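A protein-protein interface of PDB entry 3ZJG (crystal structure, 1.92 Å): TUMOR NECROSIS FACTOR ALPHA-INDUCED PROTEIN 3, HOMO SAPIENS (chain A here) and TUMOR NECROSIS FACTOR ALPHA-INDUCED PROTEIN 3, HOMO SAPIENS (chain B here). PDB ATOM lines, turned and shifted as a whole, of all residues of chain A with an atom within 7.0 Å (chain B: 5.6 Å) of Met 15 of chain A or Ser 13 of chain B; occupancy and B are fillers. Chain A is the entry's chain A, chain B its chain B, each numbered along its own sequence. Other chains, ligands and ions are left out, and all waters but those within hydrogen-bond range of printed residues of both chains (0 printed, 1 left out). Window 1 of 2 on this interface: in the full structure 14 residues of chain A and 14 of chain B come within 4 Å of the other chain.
OD1 of Asn 14 of chain B sits close to OD1 of Asn 14 of chain A (3.4 Å). N of Met 15 of chain A is in hydrogen-bond range of O of Ser 13 of chain B (3.4 Å). The backbone NH of Arg 16 of chain A is in hydrogen-bond range of the backbone carbonyl oxygen of Ser 13 of chain B (3.2 Å). OD1 of Asp 344 of chain B lies within salt-bridge range of NE of Arg 16 of chain A. O of Leu 12 of chain A sits close to SD of Met 15 of chain B, at 3.2 Å. The backbone carbonyl oxygen of Leu 12 of chain B sits close to the side-chain sulfur of Met 15 of chain A (3.2 Å).
The side-chain hydroxyl (OG) of Ser 13 of chain A lies close to the backbone carbonyl oxygen (O) of Leu 10 of chain A (3.3 Å). The side-chain amide oxygen (OD1) of Asn 14 of chain A sits close to the backbone NH (N) of Arg 16 of chain A (3.5 Å). The backbone NH (N) of Lys 17 of chain A lies within hydrogen-bond range of the side-chain amide oxygen (OD1) of Asn 14 of chain A. The side-chain hydroxyl of Tyr 345 of chain B sits at hydrogen-bond distance from the backbone carbonyl oxygen of Pro 7 of chain B. The backbone NH (N) of Tyr 345 of chain B is in hydrogen-bond range of the side-chain hydroxyl (OG) of Ser 13 of chain B (3.1 Å). The side-chain amide nitrogen (ND2) of Asn 14 of chain B sits at hydrogen-bond distance from the side-chain carboxylate (OD2) of Asp 344 of chain B, at 3.2 Å.
Hydrophobic or aromatic side chains of chain A that line the printed part of chain B: Leu 12, Met 15 and Val 19. Of the 14 printed residues of chain B, 7 touch a printed residue of chain A. Hydrophobic or aromatic side chains of chain B that line the printed part of chain A: Pro 7, Leu 12, Met 15 and Leu 348. Among the printed residues, Asp or Glu carboxylates within 4 Å of a Lys or Arg side-chain nitrogen of the other chain: Arg 16 of chain A with Asp 344 of chain B.
Among the printed residues, merely in contact across the chains: Val 19 of chain A with Leu 348 of chain B (3.5 Å), Met 15 of chain A with Leu 348 of chain B (3.5 Å), Ser 13 of chain A with Met 15 of chain B (3.6 Å), Met 15 of chain A with Pro 7 of chain B (3.6 Å), Leu 12 of chain A with Leu 12 of chain B (3.8 Å) and Arg 16 of chain A with Leu 348 of chain B (3.995 Å).
Printed residues of chain B within 4 Å of Ser 13 of chain A: Met 15. Of the printed residues of chain B, Arg 16 of chain A touches Ser 13 (3.2 Å), Asp 344 (3.0 Å) and Leu 348 (3.995 Å). Val 5 of chain B touches none of the printed residues of chain A. Printed residues of chain A within 4 Å of Leu 12 of chain B: Leu 12 and Met 15. Of chain A, only Met 15 (3.4 Å) and Arg 16 (3.2 Å) come within 4 Å of Ser 13 of chain B. Printed residues of chain A within 4 Å of Asp 344 of chain B: Arg 16. Of the printed residues of chain A, Leu 348 of chain B touches Met 15, Arg 16 and Val 19. The nearest residue of chain A that does not touch Ser 13 of chain B is Asn 14 of chain A (4.3 Å).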
ATOM      1  N   LEU A  10      -9.240  -7.683  -8.891  1.00  0.00           N
ATOM      2  CA  LEU A  10      -8.447  -6.552  -8.438  1.00  0.00           C
ATOM      3  C   LEU A  10      -7.898  -6.720  -7.051  1.00  0.00           C
ATOM      4  O   LEU A  10      -6.723  -6.436  -6.815  1.00  0.00           O
ATOM      5  CB  LEU A  10      -9.273  -5.278  -8.479  1.00  0.00           C
ATOM      6  CG  LEU A  10      -8.681  -3.992  -7.934  1.00  0.00           C
ATOM      7  CD1 LEU A  10      -7.438  -3.665  -8.619  1.00  0.00           C
ATOM      8  CD2 LEU A  10      -9.772  -2.912  -8.316  1.00  0.00           C
ATOM      9  N   TYR A  11      -8.729  -7.173  -6.116  1.00  0.00           N
ATOM     10  CA  TYR A  11      -8.268  -7.171  -4.726  1.00  0.00           C
ATOM     11  C   TYR A  11      -7.248  -8.237  -4.419  1.00  0.00           C
ATOM     12  O   TYR A  11      -6.546  -8.161  -3.430  1.00  0.00           O
ATOM     13  CB  TYR A  11      -9.416  -7.224  -3.714  1.00  0.00           C
ATOM     14  CG  TYR A  11     -10.635  -8.017  -4.135  1.00  0.00           C
ATOM     15  CD1 TYR A  11     -10.648  -9.421  -4.058  1.00  0.00           C
ATOM     16  CD2 TYR A  11     -11.804  -7.346  -4.587  1.00  0.00           C
ATOM     17  CE1 TYR A  11     -11.795 -10.156  -4.436  1.00  0.00           C
ATOM     18  CE2 TYR A  11     -12.952  -8.051  -4.959  1.00  0.00           C
ATOM     19  CZ  TYR A  11     -12.949  -9.460  -4.880  1.00  0.00           C
ATOM     20  OH  TYR A  11     -14.095 -10.148  -5.248  1.00  0.00           O
ATOM     21  N   LEU A  12      -7.152  -9.243  -5.268  1.00  0.00           N
ATOM     22  CA  LEU A  12      -6.164 -10.255  -5.006  1.00  0.00           C
ATOM     23  C   LEU A  12      -4.767  -9.644  -5.195  1.00  0.00           C
ATOM     24  O   LEU A  12      -3.774 -10.301  -4.946  1.00  0.00           O
ATOM     25  CB  LEU A  12      -6.400 -11.459  -5.922  1.00  0.00           C
ATOM     26  CG  LEU A  12      -7.234 -12.576  -5.297  1.00  0.00           C
ATOM     27  CD1 LEU A  12      -8.280 -12.025  -4.310  1.00  0.00           C
ATOM     28  CD2 LEU A  12      -7.881 -13.423  -6.386  1.00  0.00           C
ATOM     29  N   SER A  13      -4.687  -8.385  -5.623  1.00  0.00           N
ATOM     30  CA  SER A  13      -3.380  -7.810  -5.926  1.00  0.00           C
ATOM     31  C   SER A  13      -2.603  -7.378  -4.661  1.00  0.00           C
ATOM     32  O   SER A  13      -1.374  -7.339  -4.643  1.00  0.00           O
ATOM     33  CB  SER A  13      -3.519  -6.680  -6.968  1.00  0.00           C
ATOM     34  OG  SER A  13      -3.572  -5.396  -6.381  1.00  0.00           O
ATOM     35  N   ASN A  14      -3.320  -7.051  -3.601  1.00  0.00           N
ATOM     36  CA  ASN A  14      -2.684  -6.713  -2.318  1.00  0.00           C
ATOM     37  C   ASN A  14      -3.722  -6.859  -1.208  1.00  0.00           C
ATOM     38  O   ASN A  14      -4.327  -5.858  -0.776  1.00  0.00           O
ATOM     39  CB  ASN A  14      -2.054  -5.302  -2.336  1.00  0.00           C
ATOM     40  CG  ASN A  14      -1.131  -5.028  -1.130  1.00  0.00           C
ATOM     41  OD1 ASN A  14      -1.250  -5.647  -0.082  1.00  0.00           O
ATOM     42  ND2 ASN A  14      -0.225  -4.072  -1.280  1.00  0.00           N
ATOM     43  N   MET A  15      -3.977  -8.108  -0.798  1.00  0.00           N
ATOM     44  CA  MET A  15      -4.977  -8.371   0.237  1.00  0.00           C
ATOM     45  C   MET A  15      -4.689  -7.601   1.541  1.00  0.00           C
ATOM     46  O   MET A  15      -5.606  -7.044   2.155  1.00  0.00           O
ATOM     47  CB  MET A  15      -5.219  -9.858   0.465  1.00  0.00           C
ATOM     48  CG  MET A  15      -5.559 -10.685  -0.771  1.00  0.00           C
ATOM     49  SD  MET A  15      -6.104 -12.364  -0.335  1.00  0.00           S
ATOM     50  CE  MET A  15      -7.553 -11.958   0.658  1.00  0.00           C
ATOM     51  N   ARG A  16      -3.423  -7.483   1.927  1.00  0.00           N
ATOM     52  CA  ARG A  16      -3.048  -6.725   3.130  1.00  0.00           C
ATOM     53  C   ARG A  16      -3.441  -5.248   3.029  1.00  0.00           C
ATOM     54  O   ARG A  16      -4.038  -4.676   3.958  1.00  0.00           O
ATOM     55  CB  ARG A  16      -1.539  -6.900   3.432  1.00  0.00           C
ATOM     56  CG  ARG A  16      -1.027  -6.165   4.663  1.00  0.00           C
ATOM     57  CD  ARG A  16      -1.906  -6.411   5.872  1.00  0.00           C
ATOM     58  NE  ARG A  16      -1.437  -5.751   7.091  1.00  0.00           N
ATOM     59  CZ  ARG A  16      -1.705  -4.493   7.437  1.00  0.00           C
ATOM     60  NH1 ARG A  16      -2.419  -3.721   6.655  1.00  0.00           N
ATOM     61  NH2 ARG A  16      -1.237  -4.002   8.572  1.00  0.00           N
ATOM     62  N   LYS A  17      -3.151  -4.625   1.891  1.00  0.00           N
ATOM     63  CA  LYS A  17      -3.519  -3.201   1.704  1.00  0.00           C
ATOM     64  C   LYS A  17      -5.052  -3.001   1.712  1.00  0.00           C
ATOM     65  O   LYS A  17      -5.548  -2.023   2.262  1.00  0.00           O
ATOM     66  CB  LYS A  17      -2.869  -2.646   0.416  1.00  0.00           C
ATOM     67  CG  LYS A  17      -3.014  -1.118   0.152  1.00  0.00           C
ATOM     68  CD  LYS A  17      -2.353  -0.694  -1.181  1.00  0.00           C
ATOM     69  CE  LYS A  17      -0.863  -0.413  -1.019  1.00  0.00           C
ATOM     70  NZ  LYS A  17      -0.157  -0.372  -2.330  1.00  0.00           N
ATOM     71  N   ALA A  18      -5.802  -3.928   1.128  1.00  0.00           N
ATOM     72  CA  ALA A  18      -7.257  -3.838   1.137  1.00  0.00           C
ATOM     73  C   ALA A  18      -7.801  -3.739   2.563  1.00  0.00           C
ATOM     74  O   ALA A  18      -8.596  -2.869   2.890  1.00  0.00           O
ATOM     75  CB  ALA A  18      -7.839  -5.016   0.439  1.00  0.00           C
ATOM     76  N   VAL A  19      -7.362  -4.652   3.415  1.00  0.00           N
ATOM     77  CA  VAL A  19      -7.689  -4.577   4.815  1.00  0.00           C
ATOM     78  C   VAL A  19      -7.307  -3.247   5.483  1.00  0.00           C
ATOM     79  O   VAL A  19      -8.092  -2.714   6.255  1.00  0.00           O
ATOM     80  CB  VAL A  19      -7.078  -5.781   5.594  1.00  0.00           C
ATOM     81  CG1 VAL A  19      -6.955  -5.458   7.087  1.00  0.00           C
ATOM     82  CG2 VAL A  19      -7.934  -7.015   5.352  1.00  0.00           C
ATOM     83  N   LYS A  20      -6.103  -2.743   5.227  1.00  0.00           N
ATOM     84  CA  LYS A  20      -5.657  -1.470   5.807  1.00  0.00           C
ATOM     85  C   LYS A  20      -6.690  -0.433   5.397  1.00  0.00           C
ATOM     86  O   LYS A  20      -7.241   0.286   6.230  1.00  0.00           O
ATOM     87  CB  LYS A  20      -4.300  -1.058   5.216  1.00  0.00           C
ATOM     88  CG  LYS A  20      -3.427  -0.056   6.004  1.00  0.00           C
ATOM     89  CD  LYS A  20      -4.079   1.279   6.336  1.00  0.00           C
ATOM     90  CE  LYS A  20      -4.298   1.466   7.851  1.00  0.00           C
ATOM     91  NZ  LYS A  20      -3.825   2.810   8.353  1.00  0.00           N
ATOM     92  N   ARG A  22      -9.864  -0.630   4.283  1.00  0.00           N
ATOM     93  CA  ARG A  22     -11.088  -0.864   5.031  1.00  0.00           C
ATOM     94  C   ARG A  22     -11.012  -0.508   6.518  1.00  0.00           C
ATOM     95  O   ARG A  22     -11.899   0.186   7.021  1.00  0.00           O
ATOM     96  CB  ARG A  22     -11.603  -2.276   4.756  1.00  0.00           C
ATOM     97  CG  ARG A  22     -11.907  -2.399   3.228  1.00  0.00           C
ATOM     98  CD  ARG A  22     -12.967  -3.405   2.904  1.00  0.00           C
ATOM     99  NE  ARG A  22     -12.394  -4.716   3.135  1.00  0.00           N
ATOM    100  CZ  ARG A  22     -11.822  -5.460   2.190  1.00  0.00           C
ATOM    101  NH1 ARG A  22     -11.818  -5.054   0.912  1.00  0.00           N
ATOM    102  NH2 ARG A  22     -11.290  -6.640   2.519  1.00  0.00           N
ATOM    103  N   LEU A 341      -5.282  -0.085  -4.698  1.00  0.00           N
ATOM    104  CA  LEU A 341      -5.081  -1.432  -5.231  1.00  0.00           C
ATOM    105  C   LEU A 341      -4.835  -1.376  -6.733  1.00  0.00           C
ATOM    106  O   LEU A 341      -4.202  -2.253  -7.302  1.00  0.00           O
ATOM    107  CB  LEU A 341      -6.299  -2.312  -4.953  1.00  0.00           C
ATOM    108  CG  LEU A 341      -6.527  -2.659  -3.475  1.00  0.00           C
ATOM    109  CD1 LEU A 341      -7.624  -3.750  -3.280  1.00  0.00           C
ATOM    110  CD2 LEU A 341      -5.205  -3.064  -2.851  1.00  0.00           C
ATOM    111  N   VAL B   5     -12.376 -16.935   2.687  1.00  0.00           N
ATOM    112  CA  VAL B   5     -12.140 -15.497   2.851  1.00  0.00           C
ATOM    113  C   VAL B   5     -10.665 -15.205   3.168  1.00  0.00           C
ATOM    114  O   VAL B   5     -10.155 -14.120   2.866  1.00  0.00           O
ATOM    115  CB  VAL B   5     -13.058 -14.878   3.939  1.00  0.00           C
ATOM    116  N   LEU B   6      -9.984 -16.174   3.777  1.00  0.00           N
ATOM    117  CA  LEU B   6      -8.524 -16.112   3.915  1.00  0.00           C
ATOM    118  C   LEU B   6      -7.813 -16.337   2.569  1.00  0.00           C
ATOM    119  O   LEU B   6      -8.458 -16.647   1.572  1.00  0.00           O
ATOM    120  CB  LEU B   6      -8.037 -17.118   4.955  1.00  0.00           C
ATOM    121  CG  LEU B   6      -8.281 -16.672   6.397  1.00  0.00           C
ATOM    122  CD1 LEU B   6      -7.732 -17.686   7.386  1.00  0.00           C
ATOM    123  CD2 LEU B   6      -7.651 -15.321   6.652  1.00  0.00           C
ATOM    124  N   PRO B   7      -6.489 -16.136   2.520  1.00  0.00           N
ATOM    125  CA  PRO B   7      -5.837 -16.496   1.259  1.00  0.00           C
ATOM    126  C   PRO B   7      -5.529 -17.990   1.154  1.00  0.00           C
ATOM    127  O   PRO B   7      -4.828 -18.572   1.998  1.00  0.00           O
ATOM    128  CB  PRO B   7      -4.548 -15.662   1.271  1.00  0.00           C
ATOM    129  CG  PRO B   7      -4.831 -14.560   2.241  1.00  0.00           C
ATOM    130  CD  PRO B   7      -5.668 -15.201   3.300  1.00  0.00           C
ATOM    131  N   ALA B   9      -3.602 -19.657  -0.353  1.00  0.00           N
ATOM    132  CA  ALA B   9      -2.177 -19.965  -0.344  1.00  0.00           C
ATOM    133  C   ALA B   9      -1.445 -18.757   0.254  1.00  0.00           C
ATOM    134  O   ALA B   9      -2.020 -17.679   0.328  1.00  0.00           O
ATOM    135  CB  ALA B   9      -1.710 -20.200  -1.779  1.00  0.00           C
ATOM    136  N   LEU B  10      -0.180 -18.900   0.642  1.00  0.00           N
ATOM    137  CA  LEU B  10       0.562 -17.746   1.179  1.00  0.00           C
ATOM    138  C   LEU B  10       0.753 -16.574   0.212  1.00  0.00           C
ATOM    139  O   LEU B  10       0.527 -15.422   0.585  1.00  0.00           O
ATOM    140  CB  LEU B  10       1.931 -18.159   1.620  1.00  0.00           C
ATOM    141  CG  LEU B  10       2.687 -17.223   2.572  1.00  0.00           C
ATOM    142  CD1 LEU B  10       1.748 -16.794   3.634  1.00  0.00           C
ATOM    143  CD2 LEU B  10       3.836 -17.996   3.185  1.00  0.00           C
ATOM    144  N   TYR B  11       1.224 -16.862  -1.010  1.00  0.00           N
ATOM    145  CA  TYR B  11       1.625 -15.801  -1.928  1.00  0.00           C
ATOM    146  C   TYR B  11       0.431 -14.868  -2.211  1.00  0.00           C
ATOM    147  O   TYR B  11       0.611 -13.677  -2.515  1.00  0.00           O
ATOM    148  CB  TYR B  11       2.284 -16.362  -3.213  1.00  0.00           C
ATOM    149  CG  TYR B  11       1.306 -16.733  -4.319  1.00  0.00           C
ATOM    150  CD1 TYR B  11       0.629 -17.960  -4.298  1.00  0.00           C
ATOM    151  CD2 TYR B  11       1.057 -15.855  -5.385  1.00  0.00           C
ATOM    152  CE1 TYR B  11      -0.268 -18.296  -5.291  1.00  0.00           C
ATOM    153  CE2 TYR B  11       0.166 -16.188  -6.394  1.00  0.00           C
ATOM    154  CZ  TYR B  11      -0.496 -17.404  -6.332  1.00  0.00           C
ATOM    155  OH  TYR B  11      -1.381 -17.739  -7.315  1.00  0.00           O
ATOM    156  N   LEU B  12      -0.785 -15.403  -2.072  1.00  0.00           N
ATOM    157  CA  LEU B  12      -1.990 -14.627  -2.354  1.00  0.00           C
ATOM    158  C   LEU B  12      -2.252 -13.468  -1.362  1.00  0.00           C
ATOM    159  O   LEU B  12      -3.126 -12.613  -1.599  1.00  0.00           O
ATOM    160  CB  LEU B  12      -3.212 -15.553  -2.478  1.00  0.00           C
ATOM    161  CG  LEU B  12      -3.524 -16.032  -3.904  1.00  0.00           C
ATOM    162  CD1 LEU B  12      -4.080 -17.448  -3.905  1.00  0.00           C
ATOM    163  CD2 LEU B  12      -4.502 -15.070  -4.628  1.00  0.00           C
ATOM    164  N   SER B  13      -1.467 -13.444  -0.288  1.00  0.00           N
ATOM    165  CA  SER B  13      -1.596 -12.486   0.809  1.00  0.00           C
ATOM    166  C   SER B  13      -1.169 -11.056   0.450  1.00  0.00           C
ATOM    167  O   SER B  13      -1.763 -10.081   0.937  1.00  0.00           O
ATOM    168  CB  SER B  13      -0.782 -12.980   2.007  1.00  0.00           C
ATOM    169  OG  SER B  13      -0.723 -11.972   2.990  1.00  0.00           O
ATOM    170  N   ASN B  14      -0.151 -10.925  -0.397  1.00  0.00           N
ATOM    171  CA  ASN B  14       0.312  -9.625  -0.879  1.00  0.00           C
ATOM    172  C   ASN B  14       1.154  -9.828  -2.123  1.00  0.00           C
ATOM    173  O   ASN B  14       2.418  -9.783  -2.064  1.00  0.00           O
ATOM    174  CB  ASN B  14       1.079  -8.858   0.209  1.00  0.00           C
ATOM    175  CG  ASN B  14       1.497  -7.465  -0.219  1.00  0.00           C
ATOM    176  OD1 ASN B  14       1.487  -7.124  -1.402  1.00  0.00           O
ATOM    177  ND2 ASN B  14       1.891  -6.654   0.745  1.00  0.00           N
ATOM    178  N   MET B  15       0.442 -10.081  -3.227  1.00  0.00           N
ATOM    179  CA  MET B  15       1.054 -10.456  -4.486  1.00  0.00           C
ATOM    180  C   MET B  15       2.078  -9.411  -4.912  1.00  0.00           C
ATOM    181  O   MET B  15       3.132  -9.771  -5.413  1.00  0.00           O
ATOM    182  CB  MET B  15       0.014 -10.719  -5.599  1.00  0.00           C
ATOM    183  CG  MET B  15      -0.890 -11.925  -5.367  1.00  0.00           C
ATOM    184  SD  MET B  15      -1.955 -12.203  -6.768  1.00  0.00           S
ATOM    185  CE  MET B  15      -0.782 -12.468  -8.100  1.00  0.00           C
ATOM    186  N   LEU B 341       5.846 -12.109   3.460  1.00  0.00           N
ATOM    187  CA  LEU B 341       4.453 -12.511   3.215  1.00  0.00           C
ATOM    188  C   LEU B 341       3.752 -13.124   4.431  1.00  0.00           C
ATOM    189  O   LEU B 341       2.540 -13.068   4.546  1.00  0.00           O
ATOM    190  CB  LEU B 341       4.323 -13.476   2.035  1.00  0.00           C
ATOM    191  CG  LEU B 341       4.400 -12.946   0.605  1.00  0.00           C
ATOM    192  CD1 LEU B 341       5.818 -12.526   0.368  1.00  0.00           C
ATOM    193  CD2 LEU B 341       4.002 -14.035  -0.384  1.00  0.00           C
ATOM    194  N   ASP B 344       2.179 -10.302   6.680  1.00  0.00           N
ATOM    195  CA  ASP B 344       0.956  -9.820   6.070  1.00  0.00           C
ATOM    196  C   ASP B 344      -0.138 -10.854   6.209  1.00  0.00           C
ATOM    197  O   ASP B 344      -1.278 -10.490   6.497  1.00  0.00           O
ATOM    198  CB  ASP B 344       1.131  -9.433   4.584  1.00  0.00           C
ATOM    199  CG  ASP B 344       1.921  -8.164   4.393  1.00  0.00           C
ATOM    200  OD1 ASP B 344       1.752  -7.207   5.171  1.00  0.00           O
ATOM    201  OD2 ASP B 344       2.717  -8.112   3.438  1.00  0.00           O
ATOM    202  N   TYR B 345       0.176 -12.125   5.958  1.00  0.00           N
ATOM    203  CA  TYR B 345      -0.792 -13.212   6.191  1.00  0.00           C
ATOM    204  C   TYR B 345      -1.352 -13.122   7.600  1.00  0.00           C
ATOM    205  O   TYR B 345      -2.568 -13.210   7.813  1.00  0.00           O
ATOM    206  CB  TYR B 345      -0.176 -14.614   6.030  1.00  0.00           C
ATOM    207  CG  TYR B 345      -1.241 -15.627   5.711  1.00  0.00           C
ATOM    208  CD1 TYR B 345      -1.968 -16.231   6.712  1.00  0.00           C
ATOM    209  CD2 TYR B 345      -1.562 -15.924   4.395  1.00  0.00           C
ATOM    210  CE1 TYR B 345      -2.968 -17.117   6.436  1.00  0.00           C
ATOM    211  CE2 TYR B 345      -2.573 -16.836   4.102  1.00  0.00           C
ATOM    212  CZ  TYR B 345      -3.273 -17.425   5.143  1.00  0.00           C
ATOM    213  OH  TYR B 345      -4.296 -18.314   4.882  1.00  0.00           O
ATOM    214  N   LEU B 348      -3.801 -10.242   8.074  1.00  0.00           N
ATOM    215  CA  LEU B 348      -5.042 -10.694   7.443  1.00  0.00           C
ATOM    216  C   LEU B 348      -5.810 -11.570   8.426  1.00  0.00           C
ATOM    217  O   LEU B 348      -6.978 -11.328   8.706  1.00  0.00           O
ATOM    218  CB  LEU B 348      -4.795 -11.438   6.132  1.00  0.00           C
ATOM    219  CG  LEU B 348      -4.476 -10.562   4.911  1.00  0.00           C
ATOM    220  CD1 LEU B 348      -4.425 -11.367   3.646  1.00  0.00           C
ATOM    221  CD2 LEU B 348      -5.493  -9.432   4.760  1.00  0.00           C
